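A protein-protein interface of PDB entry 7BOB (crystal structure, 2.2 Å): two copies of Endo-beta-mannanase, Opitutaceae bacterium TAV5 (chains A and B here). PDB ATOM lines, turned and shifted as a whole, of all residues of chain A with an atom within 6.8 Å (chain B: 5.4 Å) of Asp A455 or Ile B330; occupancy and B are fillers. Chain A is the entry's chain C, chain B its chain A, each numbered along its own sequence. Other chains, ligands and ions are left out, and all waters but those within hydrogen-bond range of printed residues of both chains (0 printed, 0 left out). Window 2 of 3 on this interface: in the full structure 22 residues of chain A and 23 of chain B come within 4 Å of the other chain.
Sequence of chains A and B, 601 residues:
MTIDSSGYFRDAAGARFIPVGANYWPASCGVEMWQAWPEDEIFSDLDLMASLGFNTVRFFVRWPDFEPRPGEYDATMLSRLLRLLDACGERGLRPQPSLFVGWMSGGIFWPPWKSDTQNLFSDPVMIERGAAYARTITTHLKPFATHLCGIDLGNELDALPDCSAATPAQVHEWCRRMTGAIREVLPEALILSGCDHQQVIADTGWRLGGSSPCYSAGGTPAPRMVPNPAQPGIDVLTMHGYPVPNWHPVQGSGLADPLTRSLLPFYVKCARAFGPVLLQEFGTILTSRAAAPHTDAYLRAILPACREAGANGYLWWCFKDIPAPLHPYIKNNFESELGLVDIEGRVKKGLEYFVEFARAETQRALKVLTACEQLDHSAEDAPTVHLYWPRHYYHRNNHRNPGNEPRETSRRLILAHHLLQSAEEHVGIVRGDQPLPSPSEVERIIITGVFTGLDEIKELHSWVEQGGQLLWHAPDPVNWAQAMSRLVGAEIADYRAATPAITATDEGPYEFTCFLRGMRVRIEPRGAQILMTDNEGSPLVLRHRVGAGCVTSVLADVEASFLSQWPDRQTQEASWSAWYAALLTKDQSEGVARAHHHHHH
The side-chain amide oxygen of Asn A479 lies close to the backbone carbonyl oxygen of Ile B330 (3.2 Å). The backbone NH (N) of Asn B333 sits at hydrogen-bond distance from the backbone carbonyl oxygen (O) of Val A478 (3.3 Å). O of Lys B331 lies within hydrogen-bond range of ND2 of Asn A479 (3.0 Å). The side-chain amide oxygen of Asn A479 lies within hydrogen-bond range of the backbone NH of Asn B332, at 3.5 Å. The backbone carbonyl oxygen of Ile B330 lies within hydrogen-bond range of the backbone NH of Leu A454. The backbone NH of Asn B333 lies within hydrogen-bond range of the side-chain amide oxygen of Asn A479, 2.8 Å away.
A ring nitrogen (NE2) of His A392 sits close to the backbone carbonyl oxygen of Arg A400. ND2 of Asn B333 sits at hydrogen-bond distance from O of Tyr B329 (2.8 Å). OD2 of Asp A455 lies within salt-bridge range of NE of Arg A391. ND2 of Asn A479 is in hydrogen-bond range of O of Thr A452, 3.2 Å away. The backbone NH (N) of Gly A453 is in hydrogen-bond range of the side-chain carboxylate (OE2) of Glu A456.
Among the printed residues, merely in contact across the chains: Arg A400 with His B327, Arg A400 with Lys B331, Pro A402 with Lys B331, Gly A453 with Ile B330, Leu A454 with Asn B333, Asp A455 with Ile B330 and Val A478 with Asn B332.
Printed residues of chain B within 4 Å of Leu A454: Ile B330 and Asn B333. Of chain B, only Ile B330 comes within 4 Å of Asp A455. Ile A457 touches none of the printed residues of chain B. Lys A458 touches none of the printed residues of chain B. Of the printed residues of chain B, Asn A479 touches Ile B330, Lys B331, Asn B332 and Asn B333. Ile B330 touches four residues of chain A. Of the printed residues of chain A, Lys B331 touches Arg A400 (3.6 Å), Pro A402 (3.3 Å) and Asn A479 (3.0 Å).
Hydrophobic or aromatic side chains of chain B within 4 Å of the printed part of chain A: His B327 and Ile B330. Of the 17 printed residues of chain A, 7 touch a printed residue of chain B. Printed residues of chain A that touch a printed residue of chain B: Arg A400, Pro A402, Gly A453, Leu A454, Asp A455, Val A478 and Asn A479. Hydrophobic or aromatic side chains of chain A within 4 Å of the printed part of chain B: Pro A402, Leu A454 and Val A478. Among the printed residues, 13 pairs touch across the chains.
No position is printed for both chains.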
ATOM      1  N   TYR A 388      -3.496 -25.313   9.555  1.00  0.00           N
ATOM      2  CA  TYR A 388      -2.982 -24.305   8.632  1.00  0.00           C
ATOM      3  C   TYR A 388      -3.407 -22.922   9.093  1.00  0.00           C
ATOM      4  O   TYR A 388      -4.597 -22.592   9.066  1.00  0.00           O
ATOM      5  CB  TYR A 388      -3.465 -24.553   7.201  1.00  0.00           C
ATOM      6  CG  TYR A 388      -2.855 -23.577   6.209  1.00  0.00           C
ATOM      7  CD1 TYR A 388      -3.583 -22.485   5.736  1.00  0.00           C
ATOM      8  CD2 TYR A 388      -1.563 -23.747   5.747  1.00  0.00           C
ATOM      9  CE1 TYR A 388      -3.051 -21.600   4.820  1.00  0.00           C
ATOM     10  CE2 TYR A 388      -1.009 -22.860   4.807  1.00  0.00           C
ATOM     11  CZ  TYR A 388      -1.759 -21.787   4.365  1.00  0.00           C
ATOM     12  OH  TYR A 388      -1.223 -20.893   3.469  1.00  0.00           O
ATOM     13  N   ARG A 391      -2.059 -17.035   5.603  1.00  0.00           N
ATOM     14  CA  ARG A 391      -1.052 -15.988   5.437  1.00  0.00           C
ATOM     15  C   ARG A 391      -1.578 -14.645   5.922  1.00  0.00           C
ATOM     16  O   ARG A 391      -0.833 -13.857   6.511  1.00  0.00           O
ATOM     17  CB  ARG A 391      -0.612 -15.873   3.966  1.00  0.00           C
ATOM     18  CG  ARG A 391       0.109 -14.538   3.660  1.00  0.00           C
ATOM     19  CD  ARG A 391       0.767 -14.507   2.271  1.00  0.00           C
ATOM     20  NE  ARG A 391       1.847 -15.482   2.177  1.00  0.00           N
ATOM     21  CZ  ARG A 391       3.082 -15.291   2.641  1.00  0.00           C
ATOM     22  NH1 ARG A 391       3.423 -14.142   3.240  1.00  0.00           N
ATOM     23  NH2 ARG A 391       3.977 -16.266   2.516  1.00  0.00           N
ATOM     24  N   HIS A 392      -2.849 -14.366   5.669  1.00  0.00           N
ATOM     25  CA  HIS A 392      -3.505 -13.123   6.055  1.00  0.00           C
ATOM     26  C   HIS A 392      -4.582 -13.525   7.054  1.00  0.00           C
ATOM     27  O   HIS A 392      -5.610 -14.099   6.677  1.00  0.00           O
ATOM     28  CB  HIS A 392      -4.080 -12.404   4.834  1.00  0.00           C
ATOM     29  CG  HIS A 392      -3.061 -12.131   3.769  1.00  0.00           C
ATOM     30  ND1 HIS A 392      -2.089 -11.159   3.906  1.00  0.00           N
ATOM     31  CD2 HIS A 392      -2.851 -12.704   2.558  1.00  0.00           C
ATOM     32  CE1 HIS A 392      -1.324 -11.150   2.830  1.00  0.00           C
ATOM     33  NE2 HIS A 392      -1.769 -12.072   1.993  1.00  0.00           N
ATOM     34  N   ARG A 400      -4.826  -7.100   1.527  1.00  0.00           N
ATOM     35  CA  ARG A 400      -4.374  -8.333   0.891  1.00  0.00           C
ATOM     36  C   ARG A 400      -5.092  -9.572   1.420  1.00  0.00           C
ATOM     37  O   ARG A 400      -4.772 -10.688   1.007  1.00  0.00           O
ATOM     38  CB  ARG A 400      -2.857  -8.497   1.072  1.00  0.00           C
ATOM     39  CG  ARG A 400      -2.025  -7.296   0.549  1.00  0.00           C
ATOM     40  CD  ARG A 400      -1.121  -7.697  -0.625  1.00  0.00           C
ATOM     41  NE  ARG A 400      -0.704  -6.562  -1.468  1.00  0.00           N
ATOM     42  CZ  ARG A 400      -0.031  -6.681  -2.615  1.00  0.00           C
ATOM     43  NH1 ARG A 400       0.308  -7.889  -3.068  1.00  0.00           N
ATOM     44  NH2 ARG A 400       0.308  -5.596  -3.312  1.00  0.00           N
ATOM     45  N   PRO A 402      -7.895 -12.324   1.796  1.00  0.00           N
ATOM     46  CA  PRO A 402      -9.004 -12.838   0.985  1.00  0.00           C
ATOM     47  C   PRO A 402     -10.294 -13.064   1.753  1.00  0.00           C
ATOM     48  O   PRO A 402     -11.245 -13.583   1.171  1.00  0.00           O
ATOM     49  CB  PRO A 402      -8.455 -14.161   0.435  1.00  0.00           C
ATOM     50  CG  PRO A 402      -7.456 -14.593   1.451  1.00  0.00           C
ATOM     51  CD  PRO A 402      -6.809 -13.308   1.934  1.00  0.00           C
ATOM     52  N   GLY A 432       1.231 -20.151   7.302  1.00  0.00           N
ATOM     53  CA  GLY A 432       1.162 -19.865   5.882  1.00  0.00           C
ATOM     54  C   GLY A 432       1.780 -18.548   5.453  1.00  0.00           C
ATOM     55  O   GLY A 432       1.848 -18.289   4.250  1.00  0.00           O
ATOM     56  N   THR A 452      -7.391 -18.728   1.069  1.00  0.00           N
ATOM     57  CA  THR A 452      -6.005 -18.889   0.652  1.00  0.00           C
ATOM     58  C   THR A 452      -5.786 -18.179  -0.678  1.00  0.00           C
ATOM     59  O   THR A 452      -6.486 -18.463  -1.653  1.00  0.00           O
ATOM     60  CB  THR A 452      -5.653 -20.378   0.498  1.00  0.00           C
ATOM     61  OG1 THR A 452      -6.495 -20.961  -0.502  1.00  0.00           O
ATOM     62  CG2 THR A 452      -5.853 -21.131   1.801  1.00  0.00           C
ATOM     63  N   GLY A 453      -4.805 -17.264  -0.729  1.00  0.00           N
ATOM     64  CA  GLY A 453      -4.504 -16.573  -1.963  1.00  0.00           C
ATOM     65  C   GLY A 453      -3.690 -17.423  -2.935  1.00  0.00           C
ATOM     66  O   GLY A 453      -3.245 -18.531  -2.620  1.00  0.00           O
ATOM     67  N   LEU A 454      -3.500 -16.866  -4.142  1.00  0.00           N
ATOM     68  CA  LEU A 454      -2.702 -17.540  -5.166  1.00  0.00           C
ATOM     69  C   LEU A 454      -1.306 -17.896  -4.648  1.00  0.00           C
ATOM     70  O   LEU A 454      -0.811 -19.000  -4.899  1.00  0.00           O
ATOM     71  CB  LEU A 454      -2.593 -16.665  -6.422  1.00  0.00           C
ATOM     72  CG  LEU A 454      -1.724 -17.238  -7.551  1.00  0.00           C
ATOM     73  CD1 LEU A 454      -2.416 -18.425  -8.199  1.00  0.00           C
ATOM     74  CD2 LEU A 454      -1.402 -16.199  -8.628  1.00  0.00           C
ATOM     75  N   ASP A 455      -0.648 -16.984  -3.931  1.00  0.00           N
ATOM     76  CA  ASP A 455       0.709 -17.302  -3.483  1.00  0.00           C
ATOM     77  C   ASP A 455       0.699 -18.485  -2.526  1.00  0.00           C
ATOM     78  O   ASP A 455       1.568 -19.357  -2.601  1.00  0.00           O
ATOM     79  CB  ASP A 455       1.397 -16.079  -2.854  1.00  0.00           C
ATOM     80  CG  ASP A 455       0.543 -15.377  -1.825  1.00  0.00           C
ATOM     81  OD1 ASP A 455      -0.618 -15.804  -1.620  1.00  0.00           O
ATOM     82  OD2 ASP A 455       1.036 -14.404  -1.201  1.00  0.00           O
ATOM     83  N   GLU A 456      -0.311 -18.561  -1.655  1.00  0.00           N
ATOM     84  CA  GLU A 456      -0.433 -19.708  -0.755  1.00  0.00           C
ATOM     85  C   GLU A 456      -0.690 -20.991  -1.528  1.00  0.00           C
ATOM     86  O   GLU A 456      -0.112 -22.039  -1.217  1.00  0.00           O
ATOM     87  CB  GLU A 456      -1.554 -19.468   0.265  1.00  0.00           C
ATOM     88  CG  GLU A 456      -1.284 -18.266   1.162  1.00  0.00           C
ATOM     89  CD  GLU A 456      -2.443 -17.942   2.079  1.00  0.00           C
ATOM     90  OE1 GLU A 456      -2.549 -18.578   3.158  1.00  0.00           O
ATOM     91  OE2 GLU A 456      -3.249 -17.052   1.725  1.00  0.00           O
ATOM     92  N   ILE A 457      -1.546 -20.924  -2.549  1.00  0.00           N
ATOM     93  CA  ILE A 457      -1.832 -22.119  -3.335  1.00  0.00           C
ATOM     94  C   ILE A 457      -0.564 -22.622  -4.006  1.00  0.00           C
ATOM     95  O   ILE A 457      -0.240 -23.813  -3.947  1.00  0.00           O
ATOM     96  CB  ILE A 457      -2.943 -21.838  -4.357  1.00  0.00           C
ATOM     97  CG1 ILE A 457      -4.240 -21.459  -3.645  1.00  0.00           C
ATOM     98  CG2 ILE A 457      -3.166 -23.060  -5.215  1.00  0.00           C
ATOM     99  CD1 ILE A 457      -5.283 -20.848  -4.571  1.00  0.00           C
ATOM    100  N   LYS A 458       0.178 -21.714  -4.647  1.00  0.00           N
ATOM    101  CA  LYS A 458       1.428 -22.094  -5.299  1.00  0.00           C
ATOM    102  C   LYS A 458       2.397 -22.715  -4.308  1.00  0.00           C
ATOM    103  O   LYS A 458       3.063 -23.715  -4.611  1.00  0.00           O
ATOM    104  CB  LYS A 458       2.049 -20.872  -5.974  1.00  0.00           C
ATOM    105  CG  LYS A 458       1.178 -20.405  -7.159  1.00  0.00           C
ATOM    106  CD  LYS A 458       1.962 -19.726  -8.275  1.00  0.00           C
ATOM    107  CE  LYS A 458       2.335 -18.299  -7.890  1.00  0.00           C
ATOM    108  NZ  LYS A 458       2.266 -17.386  -9.076  1.00  0.00           N
ATOM    109  N   GLU A 459       2.466 -22.157  -3.104  1.00  0.00           N
ATOM    110  CA  GLU A 459       3.372 -22.724  -2.123  1.00  0.00           C
ATOM    111  C   GLU A 459       2.849 -24.068  -1.633  1.00  0.00           C
ATOM    112  O   GLU A 459       3.625 -25.005  -1.413  1.00  0.00           O
ATOM    113  CB  GLU A 459       3.569 -21.734  -0.971  1.00  0.00           C
ATOM    114  CG  GLU A 459       4.436 -22.267   0.117  1.00  0.00           C
ATOM    115  CD  GLU A 459       5.910 -22.078  -0.141  1.00  0.00           C
ATOM    116  OE1 GLU A 459       6.287 -21.739  -1.295  1.00  0.00           O
ATOM    117  OE2 GLU A 459       6.689 -22.250   0.832  1.00  0.00           O
ATOM    118  N   LEU A 460       1.530 -24.191  -1.489  1.00  0.00           N
ATOM    119  CA  LEU A 460       0.964 -25.472  -1.089  1.00  0.00           C
ATOM    120  C   LEU A 460       1.232 -26.537  -2.147  1.00  0.00           C
ATOM    121  O   LEU A 460       1.617 -27.669  -1.817  1.00  0.00           O
ATOM    122  CB  LEU A 460      -0.534 -25.321  -0.830  1.00  0.00           C
ATOM    123  CG  LEU A 460      -0.874 -24.870   0.597  1.00  0.00           C
ATOM    124  CD1 LEU A 460      -2.301 -24.359   0.657  1.00  0.00           C
ATOM    125  CD2 LEU A 460      -0.702 -26.034   1.548  1.00  0.00           C
ATOM    126  N   VAL A 478     -13.647 -18.404  -4.424  1.00  0.00           N
ATOM    127  CA  VAL A 478     -13.180 -17.065  -4.777  1.00  0.00           C
ATOM    128  C   VAL A 478     -11.717 -17.074  -5.223  1.00  0.00           C
ATOM    129  O   VAL A 478     -11.266 -16.167  -5.939  1.00  0.00           O
ATOM    130  CB  VAL A 478     -13.438 -16.125  -3.579  1.00  0.00           C
ATOM    131  CG1 VAL A 478     -12.434 -14.937  -3.519  1.00  0.00           C
ATOM    132  CG2 VAL A 478     -14.868 -15.624  -3.637  1.00  0.00           C
ATOM    133  N   ASN A 479     -10.966 -18.095  -4.839  1.00  0.00           N
ATOM    134  CA  ASN A 479      -9.607 -18.268  -5.328  1.00  0.00           C
ATOM    135  C   ASN A 479      -9.470 -19.547  -6.133  1.00  0.00           C
ATOM    136  O   ASN A 479      -8.369 -20.095  -6.248  1.00  0.00           O
ATOM    137  CB  ASN A 479      -8.621 -18.248  -4.168  1.00  0.00           C
ATOM    138  CG  ASN A 479      -8.329 -16.842  -3.699  1.00  0.00           C
ATOM    139  OD1 ASN A 479      -7.709 -16.049  -4.410  1.00  0.00           O
ATOM    140  ND2 ASN A 479      -8.816 -16.511  -2.516  1.00  0.00           N
ATOM    141  N   PRO B 325       0.547 -12.066 -11.538  1.00  0.00           N
ATOM    142  CA  PRO B 325       0.578 -12.405 -10.095  1.00  0.00           C
ATOM    143  C   PRO B 325       0.696 -11.158  -9.224  1.00  0.00           C
ATOM    144  O   PRO B 325       1.715 -10.873  -8.624  1.00  0.00           O
ATOM    145  CB  PRO B 325       1.812 -13.311 -10.001  1.00  0.00           C
ATOM    146  CG  PRO B 325       2.746 -12.754 -11.064  1.00  0.00           C
ATOM    147  CD  PRO B 325       1.862 -12.236 -12.187  1.00  0.00           C
ATOM    148  N   LEU B 326      -0.360 -10.353  -9.155  1.00  0.00           N
ATOM    149  CA  LEU B 326      -0.259  -9.132  -8.369  1.00  0.00           C
ATOM    150  C   LEU B 326      -1.640  -8.714  -7.880  1.00  0.00           C
ATOM    151  O   LEU B 326      -2.671  -9.201  -8.358  1.00  0.00           O
ATOM    152  CB  LEU B 326       0.412  -8.014  -9.166  1.00  0.00           C
ATOM    153  CG  LEU B 326      -0.141  -7.718 -10.561  1.00  0.00           C
ATOM    154  CD1 LEU B 326      -1.386  -6.869 -10.431  1.00  0.00           C
ATOM    155  CD2 LEU B 326       0.924  -7.008 -11.438  1.00  0.00           C
ATOM    156  N   HIS B 327      -1.631  -7.789  -6.917  1.00  0.00           N
ATOM    157  CA  HIS B 327      -2.846  -7.265  -6.302  1.00  0.00           C
ATOM    158  C   HIS B 327      -3.765  -6.687  -7.377  1.00  0.00           C
ATOM    159  O   HIS B 327      -3.322  -5.871  -8.186  1.00  0.00           O
ATOM    160  CB  HIS B 327      -2.458  -6.192  -5.273  1.00  0.00           C
ATOM    161  CG  HIS B 327      -3.615  -5.573  -4.541  1.00  0.00           C
ATOM    162  ND1 HIS B 327      -4.397  -6.277  -3.643  1.00  0.00           N
ATOM    163  CD2 HIS B 327      -4.083  -4.300  -4.527  1.00  0.00           C
ATOM    164  CE1 HIS B 327      -5.305  -5.467  -3.123  1.00  0.00           C
ATOM    165  NE2 HIS B 327      -5.141  -4.264  -3.646  1.00  0.00           N
ATOM    166  N   PRO B 328      -5.054  -7.052  -7.402  1.00  0.00           N
ATOM    167  CA  PRO B 328      -5.784  -7.858  -6.424  1.00  0.00           C
ATOM    168  C   PRO B 328      -6.076  -9.290  -6.902  1.00  0.00           C
ATOM    169  O   PRO B 328      -6.930  -9.969  -6.313  1.00  0.00           O
ATOM    170  CB  PRO B 328      -7.081  -7.073  -6.281  1.00  0.00           C
ATOM    171  CG  PRO B 328      -7.379  -6.670  -7.737  1.00  0.00           C
ATOM    172  CD  PRO B 328      -5.976  -6.460  -8.397  1.00  0.00           C
ATOM    173  N   TYR B 329      -5.384  -9.743  -7.953  1.00  0.00           N
ATOM    174  CA  TYR B 329      -5.598 -11.083  -8.495  1.00  0.00           C
ATOM    175  C   TYR B 329      -5.059 -12.185  -7.592  1.00  0.00           C
ATOM    176  O   TYR B 329      -5.399 -13.355  -7.820  1.00  0.00           O
ATOM    177  CB  TYR B 329      -4.957 -11.201  -9.880  1.00  0.00           C
ATOM    178  CG  TYR B 329      -5.377 -10.084 -10.804  1.00  0.00           C
ATOM    179  CD1 TYR B 329      -6.653 -10.070 -11.380  1.00  0.00           C
ATOM    180  CD2 TYR B 329      -4.518  -9.029 -11.086  1.00  0.00           C
ATOM    181  CE1 TYR B 329      -7.052  -9.028 -12.209  1.00  0.00           C
ATOM    182  CE2 TYR B 329      -4.917  -7.984 -11.920  1.00  0.00           C
ATOM    183  CZ  TYR B 329      -6.182  -7.992 -12.472  1.00  0.00           C
ATOM    184  OH  TYR B 329      -6.581  -6.958 -13.278  1.00  0.00           O
ATOM    185  N   ILE B 330      -4.231 -11.843  -6.593  1.00  0.00           N
ATOM    186  CA  ILE B 330      -3.668 -12.829  -5.675  1.00  0.00           C
ATOM    187  C   ILE B 330      -4.697 -13.241  -4.630  1.00  0.00           C
ATOM    188  O   ILE B 330      -4.900 -14.434  -4.377  1.00  0.00           O
ATOM    189  CB  ILE B 330      -2.397 -12.277  -5.006  1.00  0.00           C
ATOM    190  CG1 ILE B 330      -1.237 -12.191  -6.018  1.00  0.00           C
ATOM    191  CG2 ILE B 330      -2.027 -13.098  -3.761  1.00  0.00           C
ATOM    192  CD1 ILE B 330      -0.022 -11.331  -5.503  1.00  0.00           C
ATOM    193  N   LYS B 331      -5.362 -12.261  -4.013  1.00  0.00           N
ATOM    194  CA  LYS B 331      -6.354 -12.534  -2.975  1.00  0.00           C
ATOM    195  C   LYS B 331      -7.724 -12.944  -3.520  1.00  0.00           C
ATOM    196  O   LYS B 331      -8.512 -13.536  -2.770  1.00  0.00           O
ATOM    197  CB  LYS B 331      -6.532 -11.304  -2.084  1.00  0.00           C
ATOM    198  CG  LYS B 331      -7.334 -10.193  -2.745  1.00  0.00           C
ATOM    199  CD  LYS B 331      -7.559  -9.025  -1.812  1.00  0.00           C
ATOM    200  CE  LYS B 331      -8.754  -8.218  -2.258  1.00  0.00           C
ATOM    201  NZ  LYS B 331      -8.885  -6.980  -1.451  1.00  0.00           N
ATOM    202  N   ASN B 332      -8.049 -12.617  -4.791  1.00  0.00           N
ATOM    203  CA  ASN B 332      -9.324 -13.011  -5.418  1.00  0.00           C
ATOM    204  C   ASN B 332      -9.001 -13.617  -6.790  1.00  0.00           C
ATOM    205  O   ASN B 332      -9.293 -13.027  -7.832  1.00  0.00           O
ATOM    206  CB  ASN B 332     -10.286 -11.818  -5.553  1.00  0.00           C
ATOM    207  CG  ASN B 332     -10.987 -11.458  -4.257  1.00  0.00           C
ATOM    208  OD1 ASN B 332     -10.658 -11.974  -3.187  1.00  0.00           O
ATOM    209  ND2 ASN B 332     -11.961 -10.553  -4.344  1.00  0.00           N
ATOM    210  N   ASN B 333      -8.381 -14.799  -6.784  1.00  0.00           N
ATOM    211  CA  ASN B 333      -7.835 -15.361  -8.009  1.00  0.00           C
ATOM    212  C   ASN B 333      -8.895 -15.751  -9.039  1.00  0.00           C
ATOM    213  O   ASN B 333      -8.524 -15.953 -10.198  1.00  0.00           O
ATOM    214  CB  ASN B 333      -6.956 -16.563  -7.689  1.00  0.00           C
ATOM    215  CG  ASN B 333      -5.938 -16.852  -8.781  1.00  0.00           C
ATOM    216  OD1 ASN B 333      -5.818 -17.980  -9.230  1.00  0.00           O
ATOM    217  ND2 ASN B 333      -5.204 -15.821  -9.219  1.00  0.00           N
